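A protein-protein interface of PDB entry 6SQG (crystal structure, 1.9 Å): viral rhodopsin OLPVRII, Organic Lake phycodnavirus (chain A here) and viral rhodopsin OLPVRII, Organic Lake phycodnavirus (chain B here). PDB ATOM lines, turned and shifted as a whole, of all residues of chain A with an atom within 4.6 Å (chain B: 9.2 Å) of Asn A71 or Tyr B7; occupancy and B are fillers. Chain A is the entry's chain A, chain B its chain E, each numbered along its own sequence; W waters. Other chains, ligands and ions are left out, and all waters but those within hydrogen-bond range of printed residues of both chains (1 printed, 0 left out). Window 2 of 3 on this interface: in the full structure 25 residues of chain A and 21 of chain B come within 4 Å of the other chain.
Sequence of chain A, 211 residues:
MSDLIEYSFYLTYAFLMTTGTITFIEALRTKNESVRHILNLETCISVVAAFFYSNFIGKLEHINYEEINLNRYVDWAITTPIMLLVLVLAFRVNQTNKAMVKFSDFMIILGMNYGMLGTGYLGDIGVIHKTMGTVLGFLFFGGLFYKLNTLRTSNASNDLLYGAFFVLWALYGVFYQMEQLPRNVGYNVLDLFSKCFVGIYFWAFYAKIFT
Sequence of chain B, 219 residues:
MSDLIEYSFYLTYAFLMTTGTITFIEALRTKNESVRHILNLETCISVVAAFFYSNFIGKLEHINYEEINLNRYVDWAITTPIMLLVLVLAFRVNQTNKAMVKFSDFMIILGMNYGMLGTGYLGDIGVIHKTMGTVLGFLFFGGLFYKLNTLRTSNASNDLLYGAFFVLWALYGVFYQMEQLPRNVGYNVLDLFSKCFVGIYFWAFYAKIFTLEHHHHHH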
ATOM      1  N   PHE A  56       4.656 -39.566  -4.155  1.00  0.00           N
ATOM      2  CA  PHE A  56       3.431 -40.163  -3.619  1.00  0.00           C
ATOM      3  C   PHE A  56       3.395 -41.649  -3.882  1.00  0.00           C
ATOM      4  O   PHE A  56       3.018 -42.433  -3.010  1.00  0.00           O
ATOM      5  CB  PHE A  56       2.169 -39.551  -4.250  1.00  0.00           C
ATOM      6  CG  PHE A  56       1.989 -38.083  -3.974  1.00  0.00           C
ATOM      7  CD1 PHE A  56       2.549 -37.494  -2.866  1.00  0.00           C
ATOM      8  CD2 PHE A  56       1.229 -37.306  -4.823  1.00  0.00           C
ATOM      9  CE1 PHE A  56       2.378 -36.145  -2.620  1.00  0.00           C
ATOM     10  CE2 PHE A  56       1.052 -35.957  -4.586  1.00  0.00           C
ATOM     11  CZ  PHE A  56       1.627 -35.376  -3.482  1.00  0.00           C
ATOM     12  N   GLU A  67      -2.457 -37.447   4.653  1.00  0.00           N
ATOM     13  CA  GLU A  67      -1.117 -36.886   4.517  1.00  0.00           C
ATOM     14  C   GLU A  67      -0.789 -36.580   3.060  1.00  0.00           C
ATOM     15  O   GLU A  67      -0.128 -35.590   2.753  1.00  0.00           O
ATOM     16  CB  GLU A  67      -0.063 -37.847   5.085  1.00  0.00           C
ATOM     17  N   ILE A  68      -1.217 -37.455   2.164  1.00  0.00           N
ATOM     18  CA  ILE A  68      -0.990 -37.226   0.755  1.00  0.00           C
ATOM     19  C   ILE A  68      -1.698 -35.940   0.332  1.00  0.00           C
ATOM     20  O   ILE A  68      -1.113 -35.089  -0.335  1.00  0.00           O
ATOM     21  CB  ILE A  68      -1.486 -38.403  -0.106  1.00  0.00           C
ATOM     22  CG1 ILE A  68      -0.649 -39.653   0.165  1.00  0.00           C
ATOM     23  CG2 ILE A  68      -1.402 -38.033  -1.582  1.00  0.00           C
ATOM     24  CD1 ILE A  68      -1.200 -40.901  -0.503  1.00  0.00           C
ATOM     25  N   ASN A  69      -2.956 -35.788   0.732  1.00  0.00           N
ATOM     26  CA  ASN A  69      -3.708 -34.590   0.374  1.00  0.00           C
ATOM     27  C   ASN A  69      -3.092 -33.323   0.975  1.00  0.00           C
ATOM     28  O   ASN A  69      -3.063 -32.274   0.330  1.00  0.00           O
ATOM     29  CB  ASN A  69      -5.182 -34.726   0.759  1.00  0.00           C
ATOM     30  CG  ASN A  69      -5.939 -35.650  -0.182  1.00  0.00           C
ATOM     31  OD1 ASN A  69      -5.572 -35.806  -1.343  1.00  0.00           O
ATOM     32  ND2 ASN A  69      -6.995 -36.268   0.319  1.00  0.00           N
ATOM     33  N   LEU A  70      -2.576 -33.409   2.189  1.00  0.00           N
ATOM     34  CA  LEU A  70      -1.878 -32.253   2.759  1.00  0.00           C
ATOM     35  C   LEU A  70      -0.598 -31.947   1.956  1.00  0.00           C
ATOM     36  O   LEU A  70      -0.290 -30.789   1.688  1.00  0.00           O
ATOM     37  CB  LEU A  70      -1.574 -32.463   4.243  1.00  0.00           C
ATOM     38  CG  LEU A  70      -2.783 -32.632   5.178  1.00  0.00           C
ATOM     39  CD1 LEU A  70      -2.323 -32.897   6.605  1.00  0.00           C
ATOM     40  CD2 LEU A  70      -3.689 -31.414   5.147  1.00  0.00           C
ATOM     41  N   ASN A  71       0.120 -32.988   1.544  1.00  0.00           N
ATOM     42  CA  ASN A  71       1.362 -32.822   0.779  1.00  0.00           C
ATOM     43  C   ASN A  71       1.155 -32.199  -0.599  1.00  0.00           C
ATOM     44  O   ASN A  71       2.057 -31.562  -1.153  1.00  0.00           O
ATOM     45  CB  ASN A  71       2.045 -34.174   0.595  1.00  0.00           C
ATOM     46  CG  ASN A  71       2.689 -34.695   1.871  1.00  0.00           C
ATOM     47  OD1 ASN A  71       3.411 -35.687   1.839  1.00  0.00           O
ATOM     48  ND2 ASN A  71       2.432 -34.034   2.992  1.00  0.00           N
ATOM     49  N   ARG A  72      -0.018 -32.433  -1.177  1.00  0.00           N
ATOM     50  CA  ARG A  72      -0.350 -31.876  -2.476  1.00  0.00           C
ATOM     51  C   ARG A  72      -0.223 -30.354  -2.473  1.00  0.00           C
ATOM     52  O   ARG A  72       0.078 -29.759  -3.499  1.00  0.00           O
ATOM     53  CB  ARG A  72      -1.784 -32.240  -2.871  1.00  0.00           C
ATOM     54  CG  ARG A  72      -2.004 -33.694  -3.214  1.00  0.00           C
ATOM     55  CD  ARG A  72      -3.443 -33.938  -3.648  1.00  0.00           C
ATOM     56  NE  ARG A  72      -3.719 -35.363  -3.679  1.00  0.00           N
ATOM     57  CZ  ARG A  72      -3.581 -36.132  -4.752  1.00  0.00           C
ATOM     58  NH1 ARG A  72      -3.208 -35.614  -5.918  1.00  0.00           N
ATOM     59  NH2 ARG A  72      -3.843 -37.419  -4.658  1.00  0.00           N
ATOM     60  N   TYR A  73      -0.476 -29.721  -1.333  1.00  0.00           N
ATOM     61  CA  TYR A  73      -0.410 -28.259  -1.262  1.00  0.00           C
ATOM     62  C   TYR A  73       0.953 -27.726  -1.657  1.00  0.00           C
ATOM     63  O   TYR A  73       1.046 -26.640  -2.210  1.00  0.00           O
ATOM     64  CB  TYR A  73      -0.787 -27.733   0.126  1.00  0.00           C
ATOM     65  CG  TYR A  73      -2.265 -27.718   0.371  1.00  0.00           C
ATOM     66  CD1 TYR A  73      -3.040 -26.638  -0.022  1.00  0.00           C
ATOM     67  CD2 TYR A  73      -2.891 -28.786   0.986  1.00  0.00           C
ATOM     68  CE1 TYR A  73      -4.402 -26.623   0.190  1.00  0.00           C
ATOM     69  CE2 TYR A  73      -4.260 -28.789   1.203  1.00  0.00           C
ATOM     70  CZ  TYR A  73      -5.009 -27.700   0.815  1.00  0.00           C
ATOM     71  OH  TYR A  73      -6.365 -27.694   1.036  1.00  0.00           O
ATOM     72  N   VAL A  74       2.003 -28.482  -1.369  1.00  0.00           N
ATOM     73  CA  VAL A  74       3.350 -28.073  -1.745  1.00  0.00           C
ATOM     74  C   VAL A  74       3.499 -28.041  -3.265  1.00  0.00           C
ATOM     75  O   VAL A  74       4.028 -27.079  -3.822  1.00  0.00           O
ATOM     76  CB  VAL A  74       4.411 -28.981  -1.105  1.00  0.00           C
ATOM     77  CG1 VAL A  74       5.807 -28.474  -1.421  1.00  0.00           C
ATOM     78  CG2 VAL A  74       4.194 -29.042   0.397  1.00  0.00           C
ATOM     79  N   ASP A  75       3.013 -29.091  -3.926  1.00  0.00           N
ATOM     80  CA  ASP A  75       2.938 -29.143  -5.376  1.00  0.00           C
ATOM     81  C   ASP A  75       2.118 -27.974  -5.906  1.00  0.00           C
ATOM     82  O   ASP A  75       2.563 -27.251  -6.807  1.00  0.00           O
ATOM     83  CB  ASP A  75       2.346 -30.493  -5.805  1.00  0.00           C
ATOM     84  CG  ASP A  75       1.892 -30.529  -7.266  1.00  0.00           C
ATOM     85  OD1 ASP A  75       1.585 -29.460  -7.858  1.00  0.00           O
ATOM     86  OD2 ASP A  75       1.801 -31.661  -7.815  1.00  0.00           O
ATOM     87  N   TYR A 121      -6.009 -24.828   2.849  1.00  0.00           N
ATOM     88  CA  TYR A 121      -5.066 -25.495   3.735  1.00  0.00           C
ATOM     89  C   TYR A 121      -5.426 -25.335   5.215  1.00  0.00           C
ATOM     90  O   TYR A 121      -5.430 -26.310   5.973  1.00  0.00           O
ATOM     91  CB  TYR A 121      -3.652 -24.953   3.509  1.00  0.00           C
ATOM     92  CG  TYR A 121      -2.611 -25.650   4.355  1.00  0.00           C
ATOM     93  CD1 TYR A 121      -2.286 -26.974   4.120  1.00  0.00           C
ATOM     94  CD2 TYR A 121      -1.953 -24.989   5.385  1.00  0.00           C
ATOM     95  CE1 TYR A 121      -1.342 -27.626   4.884  1.00  0.00           C
ATOM     96  CE2 TYR A 121      -1.004 -25.638   6.156  1.00  0.00           C
ATOM     97  CZ  TYR A 121      -0.702 -26.957   5.896  1.00  0.00           C
ATOM     98  OH  TYR A 121       0.240 -27.631   6.652  1.00  0.00           O
ATOM     99  N   MET B   1       4.714 -26.420  12.181  1.00  0.00           N
ATOM    100  CA  MET B   1       4.421 -27.861  12.415  1.00  0.00           C
ATOM    101  C   MET B   1       5.675 -28.679  12.149  1.00  0.00           C
ATOM    102  O   MET B   1       6.694 -28.146  11.711  1.00  0.00           O
ATOM    103  CB  MET B   1       3.317 -28.353  11.473  1.00  0.00           C
ATOM    104  CG  MET B   1       2.456 -27.259  10.860  1.00  0.00           C
ATOM    105  SD  MET B   1       1.257 -27.902   9.672  1.00  0.00           S
ATOM    106  CE  MET B   1       0.349 -29.055  10.698  1.00  0.00           C
ATOM    107  N   SER B   2       5.595 -29.978  12.418  1.00  0.00           N
ATOM    108  CA  SER B   2       6.576 -30.914  11.892  1.00  0.00           C
ATOM    109  C   SER B   2       6.427 -30.908  10.376  1.00  0.00           C
ATOM    110  O   SER B   2       7.411 -30.965   9.641  1.00  0.00           O
ATOM    111  CB  SER B   2       6.341 -32.309  12.449  1.00  0.00           C
ATOM    112  N   ASP B   3       5.177 -30.819   9.923  1.00  0.00           N
ATOM    113  CA  ASP B   3       4.857 -30.775   8.498  1.00  0.00           C
ATOM    114  C   ASP B   3       5.566 -29.639   7.749  1.00  0.00           C
ATOM    115  O   ASP B   3       6.198 -29.873   6.720  1.00  0.00           O
ATOM    116  CB  ASP B   3       3.339 -30.651   8.294  1.00  0.00           C
ATOM    117  CG  ASP B   3       2.593 -31.949   8.586  1.00  0.00           C
ATOM    118  OD1 ASP B   3       3.253 -32.983   8.820  1.00  0.00           O
ATOM    119  OD2 ASP B   3       1.341 -31.934   8.577  1.00  0.00           O
ATOM    120  N   LEU B   4       5.449 -28.411   8.246  1.00  0.00           N
ATOM    121  CA  LEU B   4       5.973 -27.253   7.518  1.00  0.00           C
ATOM    122  C   LEU B   4       7.503 -27.228   7.445  1.00  0.00           C
ATOM    123  O   LEU B   4       8.067 -26.601   6.550  1.00  0.00           O
ATOM    124  CB  LEU B   4       5.456 -25.936   8.114  1.00  0.00           C
ATOM    125  CG  LEU B   4       3.986 -25.579   7.862  1.00  0.00           C
ATOM    126  CD1 LEU B   4       3.688 -24.202   8.437  1.00  0.00           C
ATOM    127  CD2 LEU B   4       3.630 -25.618   6.382  1.00  0.00           C
ATOM    128  N   ILE B   5       8.176 -27.902   8.374  1.00  0.00           N
ATOM    129  CA  ILE B   5       9.640 -27.992   8.329  1.00  0.00           C
ATOM    130  C   ILE B   5      10.102 -28.857   7.155  1.00  0.00           C
ATOM    131  O   ILE B   5      10.962 -28.464   6.366  1.00  0.00           O
ATOM    132  CB  ILE B   5      10.199 -28.601   9.624  1.00  0.00           C
ATOM    133  CG1 ILE B   5       9.878 -27.695  10.820  1.00  0.00           C
ATOM    134  CG2 ILE B   5      11.701 -28.818   9.499  1.00  0.00           C
ATOM    135  CD1 ILE B   5       9.880 -28.422  12.150  1.00  0.00           C
ATOM    136  N   GLU B   6       9.532 -30.052   7.061  1.00  0.00           N
ATOM    137  CA  GLU B   6       9.797 -30.951   5.950  1.00  0.00           C
ATOM    138  C   GLU B   6       9.332 -30.320   4.637  1.00  0.00           C
ATOM    139  O   GLU B   6       9.988 -30.440   3.606  1.00  0.00           O
ATOM    140  CB  GLU B   6       9.066 -32.277   6.188  1.00  0.00           C
ATOM    141  CG  GLU B   6       8.978 -33.187   4.974  1.00  0.00           C
ATOM    142  CD  GLU B   6       8.248 -34.483   5.275  1.00  0.00           C
ATOM    143  OE1 GLU B   6       8.608 -35.139   6.277  1.00  0.00           O
ATOM    144  OE2 GLU B   6       7.319 -34.843   4.515  1.00  0.00           O
ATOM    145  N   TYR B   7       8.188 -29.653   4.682  1.00  0.00           N
ATOM    146  CA  TYR B   7       7.634 -29.011   3.508  1.00  0.00           C
ATOM    147  C   TYR B   7       8.611 -27.974   2.943  1.00  0.00           C
ATOM    148  O   TYR B   7       8.706 -27.815   1.738  1.00  0.00           O
ATOM    149  CB  TYR B   7       6.299 -28.339   3.842  1.00  0.00           C
ATOM    150  CG  TYR B   7       5.083 -29.266   3.933  1.00  0.00           C
ATOM    151  CD1 TYR B   7       5.210 -30.654   3.881  1.00  0.00           C
ATOM    152  CD2 TYR B   7       3.806 -28.735   4.112  1.00  0.00           C
ATOM    153  CE1 TYR B   7       4.094 -31.480   3.988  1.00  0.00           C
ATOM    154  CE2 TYR B   7       2.691 -29.548   4.219  1.00  0.00           C
ATOM    155  CZ  TYR B   7       2.839 -30.917   4.159  1.00  0.00           C
ATOM    156  OH  TYR B   7       1.722 -31.710   4.265  1.00  0.00           O
ATOM    157  N   SER B   8       9.343 -27.282   3.814  1.00  0.00           N
ATOM    158  CA  SER B   8      10.289 -26.268   3.364  1.00  0.00           C
ATOM    159  C   SER B   8      11.417 -26.884   2.523  1.00  0.00           C
ATOM    160  O   SER B   8      11.875 -26.277   1.545  1.00  0.00           O
ATOM    161  CB  SER B   8      10.839 -25.446   4.550  1.00  0.00           C
ATOM    162  OG  SER B   8      11.715 -26.197   5.382  1.00  0.00           O
ATOM    163  N   PHE B   9      11.871 -28.074   2.901  1.00  0.00           N
ATOM    164  CA  PHE B   9      12.860 -28.789   2.101  1.00  0.00           C
ATOM    165  C   PHE B   9      12.301 -29.144   0.725  1.00  0.00           C
ATOM    166  O   PHE B   9      12.960 -28.938  -0.293  1.00  0.00           O
ATOM    167  CB  PHE B   9      13.333 -30.047   2.830  1.00  0.00           C
ATOM    168  CG  PHE B   9      14.228 -29.759   4.001  1.00  0.00           C
ATOM    169  CD1 PHE B   9      15.586 -29.575   3.813  1.00  0.00           C
ATOM    170  CD2 PHE B   9      13.711 -29.662   5.286  1.00  0.00           C
ATOM    171  CE1 PHE B   9      16.422 -29.306   4.880  1.00  0.00           C
ATOM    172  CE2 PHE B   9      14.544 -29.392   6.365  1.00  0.00           C
ATOM    173  CZ  PHE B   9      15.901 -29.213   6.160  1.00  0.00           C
ATOM    174  N   TYR B  10      11.083 -29.665   0.692  1.00  0.00           N
ATOM    175  CA  TYR B  10      10.476 -30.061  -0.575  1.00  0.00           C
ATOM    176  C   TYR B  10      10.192 -28.873  -1.473  1.00  0.00           C
ATOM    177  O   TYR B  10      10.345 -28.968  -2.689  1.00  0.00           O
ATOM    178  CB  TYR B  10       9.189 -30.858  -0.332  1.00  0.00           C
ATOM    179  CG  TYR B  10       9.436 -32.311   0.002  1.00  0.00           C
ATOM    180  CD1 TYR B  10       9.650 -32.725   1.310  1.00  0.00           C
ATOM    181  CD2 TYR B  10       9.450 -33.273  -0.996  1.00  0.00           C
ATOM    182  CE1 TYR B  10       9.862 -34.060   1.614  1.00  0.00           C
ATOM    183  CE2 TYR B  10       9.662 -34.607  -0.707  1.00  0.00           C
ATOM    184  CZ  TYR B  10       9.870 -34.996   0.600  1.00  0.00           C
ATOM    185  OH  TYR B  10      10.084 -36.328   0.874  1.00  0.00           O
ATOM    186  N   LEU B  11       9.771 -27.761  -0.872  1.00  0.00           N
ATOM    187  CA  LEU B  11       9.408 -26.576  -1.624  1.00  0.00           C
ATOM    188  C   LEU B  11      10.617 -26.046  -2.389  1.00  0.00           C
ATOM    189  O   LEU B  11      10.536 -25.740  -3.572  1.00  0.00           O
ATOM    190  CB  LEU B  11       8.850 -25.494  -0.686  1.00  0.00           C
ATOM    191  CG  LEU B  11       8.487 -24.154  -1.338  1.00  0.00           C
ATOM    192  CD1 LEU B  11       7.315 -24.303  -2.300  1.00  0.00           C
ATOM    193  CD2 LEU B  11       8.165 -23.121  -0.268  1.00  0.00           C
ATOM    194  N   THR B  12      11.752 -25.960  -1.707  1.00  0.00           N
ATOM    195  CA  THR B  12      12.960 -25.457  -2.335  1.00  0.00           C
ATOM    196  C   THR B  12      13.494 -26.440  -3.371  1.00  0.00           C
ATOM    197  O   THR B  12      13.891 -26.034  -4.466  1.00  0.00           O
ATOM    198  CB  THR B  12      14.007 -25.108  -1.276  1.00  0.00           C
ATOM    199  OG1 THR B  12      13.501 -24.025  -0.478  1.00  0.00           O
ATOM    200  CG2 THR B  12      15.335 -24.699  -1.928  1.00  0.00           C
ATOM    201  N   TYR B  13      13.493 -27.724  -3.032  1.00  0.00           N
ATOM    202  CA  TYR B  13      13.918 -28.774  -3.969  1.00  0.00           C
ATOM    203  C   TYR B  13      13.122 -28.717  -5.273  1.00  0.00           C
ATOM    204  O   TYR B  13      13.691 -28.717  -6.371  1.00  0.00           O
ATOM    205  CB  TYR B  13      13.787 -30.145  -3.303  1.00  0.00           C
ATOM    206  CG  TYR B  13      14.318 -31.299  -4.113  1.00  0.00           C
ATOM    207  CD1 TYR B  13      15.514 -31.193  -4.821  1.00  0.00           C
ATOM    208  CD2 TYR B  13      13.640 -32.504  -4.158  1.00  0.00           C
ATOM    209  CE1 TYR B  13      16.001 -32.247  -5.567  1.00  0.00           C
ATOM    210  CE2 TYR B  13      14.125 -33.571  -4.893  1.00  0.00           C
ATOM    211  CZ  TYR B  13      15.306 -33.434  -5.599  1.00  0.00           C
ATOM    212  OH  TYR B  13      15.786 -34.489  -6.341  1.00  0.00           O
ATOM    213  N   ALA B  14      11.803 -28.654  -5.163  1.00  0.00           N
ATOM    214  CA  ALA B  14      10.956 -28.617  -6.348  1.00  0.00           C
ATOM    215  C   ALA B  14      11.108 -27.296  -7.118  1.00  0.00           C
ATOM    216  O   ALA B  14      11.131 -27.297  -8.336  1.00  0.00           O
ATOM    217  CB  ALA B  14       9.503 -28.872  -5.971  1.00  0.00           C
ATOM    218  N   PHE B  15      11.242 -26.171  -6.423  1.00  0.00           N
ATOM    219  CA  PHE B  15      11.475 -24.916  -7.121  1.00  0.00           C
ATOM    220  C   PHE B  15      12.857 -24.873  -7.792  1.00  0.00           C
ATOM    221  O   PHE B  15      13.017 -24.206  -8.812  1.00  0.00           O
ATOM    222  CB  PHE B  15      11.275 -23.694  -6.211  1.00  0.00           C
ATOM    223  CG  PHE B  15      10.076 -22.864  -6.572  1.00  0.00           C
ATOM    224  CD1 PHE B  15      10.008 -22.211  -7.798  1.00  0.00           C
ATOM    225  CD2 PHE B  15       9.011 -22.733  -5.690  1.00  0.00           C
ATOM    226  CE1 PHE B  15       8.902 -21.450  -8.139  1.00  0.00           C
ATOM    227  CE2 PHE B  15       7.903 -21.967  -6.023  1.00  0.00           C
ATOM    228  CZ  PHE B  15       7.848 -21.325  -7.251  1.00  0.00           C
ATOM    229  N   TYR B  53      19.905 -30.695  -1.917  1.00  0.00           N
ATOM    230  CA  TYR B  53      18.570 -30.827  -1.331  1.00  0.00           C
ATOM    231  C   TYR B  53      18.042 -32.253  -1.428  1.00  0.00           C
ATOM    232  O   TYR B  53      17.341 -32.701  -0.525  1.00  0.00           O
ATOM    233  CB  TYR B  53      17.582 -29.819  -1.930  1.00  0.00           C
ATOM    234  CG  TYR B  53      17.617 -28.517  -1.168  1.00  0.00           C
ATOM    235  CD1 TYR B  53      18.583 -27.559  -1.443  1.00  0.00           C
ATOM    236  CD2 TYR B  53      16.745 -28.285  -0.119  1.00  0.00           C
ATOM    237  CE1 TYR B  53      18.647 -26.379  -0.714  1.00  0.00           C
ATOM    238  CE2 TYR B  53      16.805 -27.112   0.621  1.00  0.00           C
ATOM    239  CZ  TYR B  53      17.758 -26.162   0.316  1.00  0.00           C
ATOM    240  OH  TYR B  53      17.814 -24.988   1.051  1.00  0.00           O
ATOM    241  N   ILE B  57      16.780 -34.300   1.793  1.00  0.00           N
ATOM    242  CA  ILE B  57      15.464 -34.939   1.820  1.00  0.00           C
ATOM    243  C   ILE B  57      15.590 -36.435   2.122  1.00  0.00           C
ATOM    244  O   ILE B  57      14.773 -36.993   2.843  1.00  0.00           O
ATOM    245  CB  ILE B  57      14.709 -34.701   0.501  1.00  0.00           C
ATOM    246  CG1 ILE B  57      14.131 -33.282   0.485  1.00  0.00           C
ATOM    247  CG2 ILE B  57      13.597 -35.724   0.309  1.00  0.00           C
ATOM    248  CD1 ILE B  57      13.691 -32.835  -0.892  1.00  0.00           C
ATOM    249  N   LEU B  60      15.666 -37.064   5.963  1.00  0.00           N
ATOM    250  CA  LEU B  60      14.639 -36.466   6.828  1.00  0.00           C
ATOM    251  C   LEU B  60      14.194 -37.366   7.983  1.00  0.00           C
ATOM    252  O   LEU B  60      13.899 -36.874   9.072  1.00  0.00           O
ATOM    253  CB  LEU B  60      13.412 -36.055   6.007  1.00  0.00           C
ATOM    254  CG  LEU B  60      13.553 -34.756   5.220  1.00  0.00           C
ATOM    255  CD1 LEU B  60      12.367 -34.574   4.290  1.00  0.00           C
ATOM    256  CD2 LEU B  60      13.683 -33.565   6.154  1.00  0.00           C
ATOM    257  N   VAL B 185      15.244 -24.057   8.475  1.00  0.00           N
ATOM    258  CA  VAL B 185      14.060 -23.580   7.783  1.00  0.00           C
ATOM    259  C   VAL B 185      14.344 -22.233   7.117  1.00  0.00           C
ATOM    260  O   VAL B 185      13.951 -22.009   5.976  1.00  0.00           O
ATOM    261  CB  VAL B 185      12.856 -23.440   8.727  1.00  0.00           C
ATOM    262  CG1 VAL B 185      11.657 -22.899   7.966  1.00  0.00           C
ATOM    263  CG2 VAL B 185      12.530 -24.773   9.369  1.00  0.00           C
ATOM    264  N   ASN B 188      16.398 -22.731   4.044  1.00  0.00           N
ATOM    265  CA  ASN B 188      15.609 -23.305   2.950  1.00  0.00           C
ATOM    266  C   ASN B 188      14.849 -22.205   2.227  1.00  0.00           C
ATOM    267  O   ASN B 188      14.792 -22.167   0.995  1.00  0.00           O
ATOM    268  CB  ASN B 188      14.612 -24.337   3.456  1.00  0.00           C
ATOM    269  CG  ASN B 188      15.272 -25.580   4.011  1.00  0.00           C
ATOM    270  OD1 ASN B 188      16.444 -25.859   3.760  1.00  0.00           O
ATOM    271  ND2 ASN B 188      14.505 -26.342   4.772  1.00  0.00           N
ATOM    272  N   VAL B 189      14.263 -21.299   3.002  1.00  0.00           N
ATOM    273  CA  VAL B 189      13.501 -20.214   2.423  1.00  0.00           C
ATOM    274  C   VAL B 189      14.417 -19.193   1.738  1.00  0.00           C
ATOM    275  O   VAL B 189      14.093 -18.668   0.675  1.00  0.00           O
ATOM    276  CB  VAL B 189      12.621 -19.525   3.482  1.00  0.00           C
ATOM    277  CG1 VAL B 189      11.973 -18.284   2.894  1.00  0.00           C
ATOM    278  CG2 VAL B 189      11.575 -20.495   4.007  1.00  0.00           C
ATOM    279  N   LEU B 192      15.407 -20.523  -1.580  1.00  0.00           N
ATOM    280  CA  LEU B 192      14.292 -20.370  -2.514  1.00  0.00           C
ATOM    281  C   LEU B 192      14.348 -18.994  -3.167  1.00  0.00           C
ATOM    282  O   LEU B 192      14.160 -18.857  -4.381  1.00  0.00           O
ATOM    283  CB  LEU B 192      12.963 -20.574  -1.785  1.00  0.00           C
ATOM    284  CG  LEU B 192      11.672 -20.327  -2.558  1.00  0.00           C
ATOM    285  CD1 LEU B 192      11.426 -21.463  -3.531  1.00  0.00           C
ATOM    286  CD2 LEU B 192      10.481 -20.174  -1.621  1.00  0.00           C
HETATM  287  O   HOH W   1       0.351 -30.252   6.677  1.00  0.00           O
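Among the printed residues, pairs that only touch across the chains: Val A74 with Tyr B7 (3.7 Å), Tyr A121 with Tyr B7 (3.9 Å) and Tyr A121 with Leu B4 (3.95 Å).
Water W1 lies within hydrogen-bond range of the side-chain hydroxyl of Tyr A121 (2.6 Å), the side-chain carboxylate of Asp B3 (2.7 Å) and the side-chain hydroxyl of Tyr B7 (3.1 Å).
OH of Tyr A73 lies within hydrogen-bond range of N of Tyr A121 (3.4 Å). The backbone carbonyl oxygen (O) of Glu A67 lies within hydrogen-bond range of the side-chain amide nitrogen (ND2) of Asn A71, 3.0 Å away.
Printed residues of chain B that touch a printed residue of chain A: Met B1, Leu B4 and Tyr B7. Hydrophobic or aromatic side chains of chain B that line the printed part of chain A: Met B1, Leu B4 and Tyr B7. Along chain B the printed residues that touch a printed residue of chain A span positions 1 to 7. Among the printed residues, 6 pairs touch across the chains. Among the printed residues, no Asp or Glu carboxylate lies within 4 Å of a Lys or Arg side-chain nitrogen of the other chain.
Asn A71 touches just one residue of chain B: Tyr B7 (2.7 Å). Of the printed residues of chain A, Leu B4 touches Tyr A121 (3.95 Å). Of the printed residues of chain B, Val A74 touches Tyr B7 (3.7 Å). Of the printed residues of chain B, Tyr A121 touches Met B1, Leu B4 and Tyr B7. Printed residues of chain A within 4 Å of Met B1: Tyr A121 (3.2 Å). Printed residues of chain B within 4 Å of Leu A70: Tyr B7 (3.3 Å). Leu B11 touches none of the printed residues of chain A. Ala B14 touches none of the printed residues of chain A. The nearest printed residue of chain A that does not touch Tyr B7 is Glu A67 (4.6 Å). The nearest printed residue of chain B that does not touch Val A74 is Leu B11 (4.1 Å).
The side-chain hydroxyl (OH) of Tyr B7 sits close to the backbone carbonyl oxygen (O) of Leu A70 (3.4 Å). The side-chain hydroxyl (OH) of Tyr B7 sits at hydrogen-bond distance from the side-chain amide nitrogen (ND2) of Asn A71, 2.7 Å away. OH of Tyr A121 sits at hydrogen-bond distance from SD of Met B1 (3.2 Å).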
